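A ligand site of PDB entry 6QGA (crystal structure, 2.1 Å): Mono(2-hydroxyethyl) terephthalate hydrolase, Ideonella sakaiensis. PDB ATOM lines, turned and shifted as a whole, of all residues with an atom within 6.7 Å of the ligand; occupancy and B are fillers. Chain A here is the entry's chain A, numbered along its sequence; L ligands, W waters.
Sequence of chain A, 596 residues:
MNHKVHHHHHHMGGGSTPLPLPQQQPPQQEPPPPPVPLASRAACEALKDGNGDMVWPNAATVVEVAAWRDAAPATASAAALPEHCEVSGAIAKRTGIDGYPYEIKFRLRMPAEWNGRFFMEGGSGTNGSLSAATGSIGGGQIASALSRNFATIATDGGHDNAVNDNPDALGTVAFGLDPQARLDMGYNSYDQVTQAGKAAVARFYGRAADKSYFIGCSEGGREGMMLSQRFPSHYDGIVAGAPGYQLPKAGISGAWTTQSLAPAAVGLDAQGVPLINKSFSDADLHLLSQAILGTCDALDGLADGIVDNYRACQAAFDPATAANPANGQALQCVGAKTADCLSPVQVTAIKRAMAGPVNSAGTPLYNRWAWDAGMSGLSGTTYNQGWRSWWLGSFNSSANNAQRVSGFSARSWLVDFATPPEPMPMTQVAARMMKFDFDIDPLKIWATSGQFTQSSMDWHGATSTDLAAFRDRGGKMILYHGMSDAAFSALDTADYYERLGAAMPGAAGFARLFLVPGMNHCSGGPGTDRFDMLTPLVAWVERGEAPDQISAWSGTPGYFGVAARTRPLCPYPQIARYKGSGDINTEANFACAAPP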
ATOM      1  N   GLY A 123       3.505  28.458   3.776  1.00  0.00           N
ATOM      2  CA  GLY A 123       2.674  27.952   2.708  1.00  0.00           C
ATOM      3  C   GLY A 123       1.269  27.647   3.155  1.00  0.00           C
ATOM      4  O   GLY A 123       0.812  28.046   4.224  1.00  0.00           O
ATOM      5  N   SER A 124       0.549  26.950   2.286  1.00  0.00           N
ATOM      6  CA  SER A 124      -0.807  26.543   2.617  1.00  0.00           C
ATOM      7  C   SER A 124      -1.291  25.459   1.661  1.00  0.00           C
ATOM      8  O   SER A 124      -0.879  25.394   0.502  1.00  0.00           O
ATOM      9  CB  SER A 124      -1.761  27.727   2.603  1.00  0.00           C
ATOM     10  OG  SER A 124      -2.229  27.958   1.325  1.00  0.00           O
ATOM     11  N   GLY A 125      -2.178  24.613   2.176  1.00  0.00           N
ATOM     12  CA  GLY A 125      -2.612  23.455   1.420  1.00  0.00           C
ATOM     13  C   GLY A 125      -1.462  22.503   1.169  1.00  0.00           C
ATOM     14  O   GLY A 125      -0.646  22.219   2.051  1.00  0.00           O
ATOM     15  N   THR A 126      -1.381  22.013  -0.064  1.00  0.00           N
ATOM     16  CA  THR A 126      -0.229  21.235  -0.496  1.00  0.00           C
ATOM     17  C   THR A 126       0.830  22.089  -1.192  1.00  0.00           C
ATOM     18  O   THR A 126       1.676  21.544  -1.883  1.00  0.00           O
ATOM     19  CB  THR A 126      -0.667  20.084  -1.409  1.00  0.00           C
ATOM     20  OG1 THR A 126      -1.434  20.594  -2.507  1.00  0.00           O
ATOM     21  CG2 THR A 126      -1.496  19.070  -0.621  1.00  0.00           C
ATOM     22  N   ASN A 127       0.799  23.402  -0.993  1.00  0.00           N
ATOM     23  CA  ASN A 127       1.690  24.377  -1.634  1.00  0.00           C
ATOM     24  C   ASN A 127       1.564  24.231  -3.158  1.00  0.00           C
ATOM     25  O   ASN A 127       0.486  23.939  -3.675  1.00  0.00           O
ATOM     26  CB  ASN A 127       3.101  24.228  -1.090  1.00  0.00           C
ATOM     27  CG  ASN A 127       3.233  24.724   0.328  1.00  0.00           C
ATOM     28  OD1 ASN A 127       2.432  25.539   0.762  1.00  0.00           O
ATOM     29  ND2 ASN A 127       4.248  24.265   1.034  1.00  0.00           N
ATOM     30  N   CYS A 217       0.411  29.701   8.794  1.00  0.00           N
ATOM     31  CA  CYS A 217      -0.745  29.072   9.401  1.00  0.00           C
ATOM     32  C   CYS A 217      -1.014  27.761   8.674  1.00  0.00           C
ATOM     33  O   CYS A 217      -0.827  27.675   7.462  1.00  0.00           O
ATOM     34  CB  CYS A 217      -2.005  29.969   9.346  1.00  0.00           C
ATOM     35  SG  CYS A 217      -3.364  29.343  10.404  1.00  0.00           S
ATOM     36  N   SER A 218      -1.436  26.766   9.439  1.00  0.00           N
ATOM     37  CA  SER A 218      -1.797  25.445   8.915  1.00  0.00           C
ATOM     38  C   SER A 218      -0.604  24.694   8.346  1.00  0.00           C
ATOM     39  O   SER A 218       0.277  24.283   9.098  1.00  0.00           O
ATOM     40  CB  SER A 218      -2.920  25.584   7.894  1.00  0.00           C
ATOM     41  OG  SER A 218      -3.569  24.349   7.738  1.00  0.00           O
ATOM     42  N   GLU A 219      -0.550  24.491   7.029  1.00  0.00           N
ATOM     43  CA  GLU A 219       0.680  23.970   6.428  1.00  0.00           C
ATOM     44  C   GLU A 219       1.864  24.885   6.730  1.00  0.00           C
ATOM     45  O   GLU A 219       2.968  24.425   7.011  1.00  0.00           O
ATOM     46  CB  GLU A 219       0.502  23.765   4.916  1.00  0.00           C
ATOM     47  CG  GLU A 219       1.789  23.730   4.102  1.00  0.00           C
ATOM     48  CD  GLU A 219       2.775  22.641   4.517  1.00  0.00           C
ATOM     49  OE1 GLU A 219       2.347  21.599   5.036  1.00  0.00           O
ATOM     50  OE2 GLU A 219       3.980  22.822   4.320  1.00  0.00           O
ATOM     51  N   GLY A 220       1.644  26.206   6.698  1.00  0.00           N
ATOM     52  CA  GLY A 220       2.669  27.140   7.121  1.00  0.00           C
ATOM     53  C   GLY A 220       2.940  27.110   8.606  1.00  0.00           C
ATOM     54  O   GLY A 220       4.027  27.458   9.049  1.00  0.00           O
ATOM     55  N   LEU A 247       0.630  16.393   9.996  1.00  0.00           N
ATOM     56  CA  LEU A 247      -0.229  16.390   8.814  1.00  0.00           C
ATOM     57  C   LEU A 247      -0.458  15.009   8.200  1.00  0.00           C
ATOM     58  O   LEU A 247      -1.569  14.759   7.732  1.00  0.00           O
ATOM     59  CB  LEU A 247       0.332  17.349   7.761  1.00  0.00           C
ATOM     60  CG  LEU A 247      -0.660  18.450   7.376  1.00  0.00           C
ATOM     61  CD1 LEU A 247      -0.027  19.603   6.592  1.00  0.00           C
ATOM     62  CD2 LEU A 247      -1.822  17.847   6.596  1.00  0.00           C
ATOM     63  N   ALA A 250      -3.714  13.477   9.120  1.00  0.00           N
ATOM     64  CA  ALA A 250      -5.004  14.127   8.868  1.00  0.00           C
ATOM     65  C   ALA A 250      -5.921  13.229   8.059  1.00  0.00           C
ATOM     66  O   ALA A 250      -7.135  13.210   8.286  1.00  0.00           O
ATOM     67  CB  ALA A 250      -4.805  15.463   8.152  1.00  0.00           C
ATOM     68  N   GLY A 251      -5.370  12.481   7.106  1.00  0.00           N
ATOM     69  CA  GLY A 251      -6.165  11.544   6.350  1.00  0.00           C
ATOM     70  C   GLY A 251      -6.742  10.440   7.199  1.00  0.00           C
ATOM     71  O   GLY A 251      -7.850   9.966   6.946  1.00  0.00           O
ATOM     72  N   TRP A 390     -14.984  20.746   6.296  1.00  0.00           N
ATOM     73  CA  TRP A 390     -13.874  19.807   6.390  1.00  0.00           C
ATOM     74  C   TRP A 390     -14.346  18.364   6.410  1.00  0.00           C
ATOM     75  O   TRP A 390     -13.911  17.564   5.571  1.00  0.00           O
ATOM     76  CB  TRP A 390     -13.024  20.152   7.607  1.00  0.00           C
ATOM     77  CG  TRP A 390     -12.231  21.367   7.312  1.00  0.00           C
ATOM     78  CD1 TRP A 390     -12.561  22.648   7.601  1.00  0.00           C
ATOM     79  CD2 TRP A 390     -11.008  21.425   6.576  1.00  0.00           C
ATOM     80  NE1 TRP A 390     -11.619  23.493   7.142  1.00  0.00           N
ATOM     81  CE2 TRP A 390     -10.646  22.767   6.496  1.00  0.00           C
ATOM     82  CE3 TRP A 390     -10.179  20.470   6.001  1.00  0.00           C
ATOM     83  CZ2 TRP A 390      -9.483  23.191   5.855  1.00  0.00           C
ATOM     84  CZ3 TRP A 390      -9.027  20.900   5.352  1.00  0.00           C
ATOM     85  CH2 TRP A 390      -8.697  22.242   5.290  1.00  0.00           C
ATOM     86  N   GLN A 403     -13.609  18.268   2.419  1.00  0.00           N
ATOM     87  CA  GLN A 403     -12.160  18.187   2.245  1.00  0.00           C
ATOM     88  C   GLN A 403     -11.636  16.795   2.581  1.00  0.00           C
ATOM     89  O   GLN A 403     -10.703  16.313   1.938  1.00  0.00           O
ATOM     90  CB  GLN A 403     -11.444  19.206   3.127  1.00  0.00           C
ATOM     91  CG  GLN A 403     -12.035  20.585   3.140  1.00  0.00           C
ATOM     92  CD  GLN A 403     -11.946  21.249   1.809  1.00  0.00           C
ATOM     93  OE1 GLN A 403     -11.208  20.810   0.929  1.00  0.00           O
ATOM     94  NE2 GLN A 403     -12.699  22.309   1.629  1.00  0.00           N
ATOM     95  N   ARG A 404     -12.239  16.140   3.569  1.00  0.00           N
ATOM     96  CA  ARG A 404     -11.758  14.883   4.101  1.00  0.00           C
ATOM     97  C   ARG A 404     -12.479  13.676   3.535  1.00  0.00           C
ATOM     98  O   ARG A 404     -12.120  12.551   3.878  1.00  0.00           O
ATOM     99  CB  ARG A 404     -11.893  14.877   5.625  1.00  0.00           C
ATOM    100  CG  ARG A 404     -11.007  15.854   6.329  1.00  0.00           C
ATOM    101  CD  ARG A 404      -9.640  15.285   6.501  1.00  0.00           C
ATOM    102  NE  ARG A 404      -8.635  16.304   6.707  1.00  0.00           N
ATOM    103  CZ  ARG A 404      -8.473  17.004   7.827  1.00  0.00           C
ATOM    104  NH1 ARG A 404      -9.281  16.830   8.854  1.00  0.00           N
ATOM    105  NH2 ARG A 404      -7.516  17.900   7.899  1.00  0.00           N
ATOM    106  N   PHE A 408      -9.214  17.711  -1.258  1.00  0.00           N
ATOM    107  CA  PHE A 408      -7.766  17.680  -1.409  1.00  0.00           C
ATOM    108  C   PHE A 408      -7.091  16.993  -0.231  1.00  0.00           C
ATOM    109  O   PHE A 408      -5.989  16.459  -0.390  1.00  0.00           O
ATOM    110  CB  PHE A 408      -7.222  19.100  -1.594  1.00  0.00           C
ATOM    111  CG  PHE A 408      -6.894  19.791  -0.301  1.00  0.00           C
ATOM    112  CD1 PHE A 408      -5.634  19.667   0.279  1.00  0.00           C
ATOM    113  CD2 PHE A 408      -7.836  20.588   0.332  1.00  0.00           C
ATOM    114  CE1 PHE A 408      -5.336  20.293   1.473  1.00  0.00           C
ATOM    115  CE2 PHE A 408      -7.539  21.223   1.518  1.00  0.00           C
ATOM    116  CZ  PHE A 408      -6.285  21.082   2.097  1.00  0.00           C
ATOM    117  N   SER A 409      -7.689  17.047   0.959  1.00  0.00           N
ATOM    118  CA  SER A 409      -7.068  16.401   2.112  1.00  0.00           C
ATOM    119  C   SER A 409      -7.028  14.888   1.930  1.00  0.00           C
ATOM    120  O   SER A 409      -5.984  14.262   2.165  1.00  0.00           O
ATOM    121  CB  SER A 409      -7.828  16.776   3.385  1.00  0.00           C
ATOM    122  OG  SER A 409      -7.234  16.227   4.541  1.00  0.00           O
ATOM    123  N   ALA A 410      -8.124  14.288   1.478  1.00  0.00           N
ATOM    124  CA  ALA A 410      -8.160  12.859   1.214  1.00  0.00           C
ATOM    125  C   ALA A 410      -7.230  12.485   0.066  1.00  0.00           C
ATOM    126  O   ALA A 410      -6.534  11.479   0.129  1.00  0.00           O
ATOM    127  CB  ALA A 410      -9.584  12.405   0.931  1.00  0.00           C
ATOM    128  N   SER A 412      -4.526  14.132  -0.823  1.00  0.00           N
ATOM    129  CA  SER A 412      -3.138  14.345  -0.416  1.00  0.00           C
ATOM    130  C   SER A 412      -2.637  13.191   0.438  1.00  0.00           C
ATOM    131  O   SER A 412      -1.478  12.795   0.307  1.00  0.00           O
ATOM    132  CB  SER A 412      -2.996  15.677   0.329  1.00  0.00           C
ATOM    133  OG  SER A 412      -1.716  15.791   0.933  1.00  0.00           O
ATOM    134  N   TRP A 413      -3.468  12.640   1.303  1.00  0.00           N
ATOM    135  CA  TRP A 413      -3.016  11.483   2.052  1.00  0.00           C
ATOM    136  C   TRP A 413      -2.648  10.346   1.114  1.00  0.00           C
ATOM    137  O   TRP A 413      -1.576   9.751   1.233  1.00  0.00           O
ATOM    138  CB  TRP A 413      -4.076  11.052   3.067  1.00  0.00           C
ATOM    139  CG  TRP A 413      -3.556  10.018   4.036  1.00  0.00           C
ATOM    140  CD1 TRP A 413      -2.982  10.260   5.233  1.00  0.00           C
ATOM    141  CD2 TRP A 413      -3.553   8.598   3.870  1.00  0.00           C
ATOM    142  NE1 TRP A 413      -2.624   9.086   5.837  1.00  0.00           N
ATOM    143  CE2 TRP A 413      -2.968   8.047   5.026  1.00  0.00           C
ATOM    144  CE3 TRP A 413      -3.997   7.737   2.875  1.00  0.00           C
ATOM    145  CZ2 TRP A 413      -2.804   6.668   5.191  1.00  0.00           C
ATOM    146  CZ3 TRP A 413      -3.837   6.370   3.056  1.00  0.00           C
ATOM    147  CH2 TRP A 413      -3.237   5.859   4.194  1.00  0.00           C
ATOM    148  N   PHE A 417       1.245  11.192   1.347  1.00  0.00           N
ATOM    149  CA  PHE A 417       1.639  10.703   2.658  1.00  0.00           C
ATOM    150  C   PHE A 417       1.660   9.180   2.765  1.00  0.00           C
ATOM    151  O   PHE A 417       2.468   8.649   3.524  1.00  0.00           O
ATOM    152  CB  PHE A 417       0.721  11.312   3.723  1.00  0.00           C
ATOM    153  CG  PHE A 417       0.723  12.820   3.717  1.00  0.00           C
ATOM    154  CD1 PHE A 417       1.910  13.535   3.545  1.00  0.00           C
ATOM    155  CD2 PHE A 417      -0.447  13.537   3.845  1.00  0.00           C
ATOM    156  CE1 PHE A 417       1.915  14.908   3.510  1.00  0.00           C
ATOM    157  CE2 PHE A 417      -0.435  14.933   3.819  1.00  0.00           C
ATOM    158  CZ  PHE A 417       0.747  15.611   3.651  1.00  0.00           C
ATOM    159  N   ALA A 487      -9.693  21.198  10.544  1.00  0.00           N
ATOM    160  CA  ALA A 487      -8.573  20.629   9.808  1.00  0.00           C
ATOM    161  C   ALA A 487      -7.563  19.987  10.744  1.00  0.00           C
ATOM    162  O   ALA A 487      -7.132  18.864  10.518  1.00  0.00           O
ATOM    163  CB  ALA A 487      -7.902  21.713   8.960  1.00  0.00           C
ATOM    164  N   PHE A 488      -7.182  20.683  11.815  1.00  0.00           N
ATOM    165  CA  PHE A 488      -6.265  20.187  12.829  1.00  0.00           C
ATOM    166  C   PHE A 488      -6.833  20.504  14.202  1.00  0.00           C
ATOM    167  O   PHE A 488      -7.397  21.576  14.426  1.00  0.00           O
ATOM    168  CB  PHE A 488      -4.856  20.789  12.665  1.00  0.00           C
ATOM    169  CG  PHE A 488      -4.317  20.662  11.279  1.00  0.00           C
ATOM    170  CD1 PHE A 488      -4.124  19.406  10.715  1.00  0.00           C
ATOM    171  CD2 PHE A 488      -3.998  21.775  10.533  1.00  0.00           C
ATOM    172  CE1 PHE A 488      -3.637  19.281   9.424  1.00  0.00           C
ATOM    173  CE2 PHE A 488      -3.493  21.659   9.252  1.00  0.00           C
ATOM    174  CZ  PHE A 488      -3.331  20.413   8.685  1.00  0.00           C
ATOM    175  N   HIS A 521     -10.654  27.466  10.895  1.00  0.00           N
ATOM    176  CA  HIS A 521      -9.316  27.136  10.424  1.00  0.00           C
ATOM    177  C   HIS A 521      -8.602  28.397   9.946  1.00  0.00           C
ATOM    178  O   HIS A 521      -8.977  28.955   8.919  1.00  0.00           O
ATOM    179  CB  HIS A 521      -9.404  26.096   9.311  1.00  0.00           C
ATOM    180  CG  HIS A 521      -8.061  25.609   8.844  1.00  0.00           C
ATOM    181  ND1 HIS A 521      -7.129  25.065   9.700  1.00  0.00           N
ATOM    182  CD2 HIS A 521      -7.489  25.610   7.613  1.00  0.00           C
ATOM    183  CE1 HIS A 521      -6.046  24.746   9.019  1.00  0.00           C
ATOM    184  NE2 HIS A 521      -6.245  25.065   7.759  1.00  0.00           N
ATOM    185  N   CYS A 522      -7.594  28.839  10.693  1.00  0.00           N
ATOM    186  CA  CYS A 522      -6.813  30.043  10.433  1.00  0.00           C
ATOM    187  C   CYS A 522      -7.592  31.368  10.473  1.00  0.00           C
ATOM    188  O   CYS A 522      -6.979  32.416  10.678  1.00  0.00           O
ATOM    189  CB  CYS A 522      -6.076  29.926   9.089  1.00  0.00           C
ATOM    190  SG  CYS A 522      -4.790  28.648   9.094  1.00  0.00           S
ATOM    191  N   SER A 523      -8.904  31.352  10.292  1.00  0.00           N
ATOM    192  CA  SER A 523      -9.711  32.566  10.288  1.00  0.00           C
ATOM    193  C   SER A 523     -11.183  32.198  10.311  1.00  0.00           C
ATOM    194  O   SER A 523     -11.550  31.030  10.180  1.00  0.00           O
ATOM    195  CB  SER A 523      -9.421  33.424   9.067  1.00  0.00           C
ATOM    196  OG  SER A 523     -10.087  32.868   7.962  1.00  0.00           O
HETATM  197  C1  LIG L   1      -4.735  18.536   4.919  1.00  0.00           C
HETATM  198  C2  LIG L   1      -3.737  24.224   4.987  1.00  0.00           C
HETATM  199  C3  LIG L   1      -4.532  20.016   4.974  1.00  0.00           C
HETATM  200  C4  LIG L   1      -3.366  20.529   4.445  1.00  0.00           C
HETATM  201  C5  LIG L   1      -3.129  21.888   4.468  1.00  0.00           C
HETATM  202  C6  LIG L   1      -4.054  22.756   5.028  1.00  0.00           C
HETATM  203  C7  LIG L   1      -5.235  22.255   5.570  1.00  0.00           C
HETATM  204  C8  LIG L   1      -5.468  20.874   5.554  1.00  0.00           C
HETATM  205  C9  LIG L   1      -4.487  26.444   4.552  1.00  0.00           C
HETATM  206  C10 LIG L   1      -5.708  27.296   4.861  1.00  0.00           C
HETATM  207  N1  LIG L   1      -4.739  25.077   4.969  1.00  0.00           N
HETATM  208  O1  LIG L   1      -4.022  17.865   4.143  1.00  0.00           O
HETATM  209  O2  LIG L   1      -5.603  18.015   5.612  1.00  0.00           O
HETATM  210  O3  LIG L   1      -2.609  24.652   4.933  1.00  0.00           O
HETATM  211  O4  LIG L   1      -5.278  28.509   5.471  1.00  0.00           O
HETATM  212  O   HOH W   1      -1.756  18.072   2.680  1.00  0.00           O
HETATM  213  O   HOH W   2      -2.412  29.423   5.670  1.00  0.00           O
HETATM  214  O   HOH W   3      -3.882  15.242   3.951  1.00  0.00           O
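Water W3 lies within hydrogen-bond range of an oxygen (O1) of the ligand (2.6 Å) and the backbone carbonyl oxygen of Ser 409 (2.9 Å).
Water W1 bridges an oxygen (O1) of the ligand (2.7 Å) and the side-chain hydroxyl of Ser 412 (2.9 Å).
Water W2 bridges the backbone carbonyl oxygen (O) of Cys 217 (3.0 Å) and an oxygen (O4) of the ligand (3.0 Å).
NE of Arg 404 is in hydrogen-bond range of OG of Ser 409 (2.6 Å).
The backbone NH of Ser 409 sits close to the backbone carbonyl oxygen of Gln 403 (3.3 Å).
OG of Ser 218 lies within hydrogen-bond range of NE2 of His 521 (2.8 Å).
The backbone carbonyl oxygen (O) of Trp 390 is in hydrogen-bond range of the backbone NH (N) of Arg 404, 3.0 Å away.
The guanidinium group (NH2) of Arg 404 sits at hydrogen-bond distance from the backbone carbonyl oxygen (O) of Ala 487 (2.8 Å).
The backbone NH (N) of Gln 403 is in hydrogen-bond range of the backbone carbonyl oxygen (O) of Trp 390 (3.2 Å).
N of Ser 124 lies within hydrogen-bond range of OD1 of Asn 127 (2.8 Å).
SG of Cys 522 forms a disulfide with SG of Cys 217, 2.1 Å away.
O2 of the ligand is in hydrogen-bond range of OG of Ser 409.
An oxygen (O3) of the ligand lies close to the side-chain hydroxyl of Ser 218, 3.0 Å away.
The backbone NH (N) of Gly 125 is in hydrogen-bond range of an oxygen (O3) of the ligand, at 2.8 Å.
The backbone NH (N) of Glu 219 sits at hydrogen-bond distance from an oxygen (O3) of the ligand (2.9 Å).
The guanidinium group of Arg 404 is in salt-bridge range of an oxygen (O2) of the ligand.
NE2 of His 521 sits at hydrogen-bond distance from N1 of the ligand.
The side-chain sulfur (SG) of Cys 522 lies within hydrogen-bond range of an oxygen (O4) of the ligand (3.7 Å).
Residues that only touch the ligand: Leu 247 (3.3 Å), Trp 390 (3.5 Å), Ser 124 (3.5 Å), Phe 408 (3.5 Å), Ala 250 (3.7 Å) and Phe 488 (3.8 Å).
Hydrophobic or aromatic side chains that line the ligand: Leu 247, Ala 250, Trp 390, Phe 408, Phe 488 and His 521.
13 residues have an atom within 4 Å of the ligand: Ser 124, Gly 125, Ser 218, Glu 219, Leu 247, Ala 250, Trp 390, Arg 404, Phe 408, Ser 409, Phe 488, His 521 and Cys 522.
Along chain A the residues within 4 Å of the ligand span positions 124 to 522.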
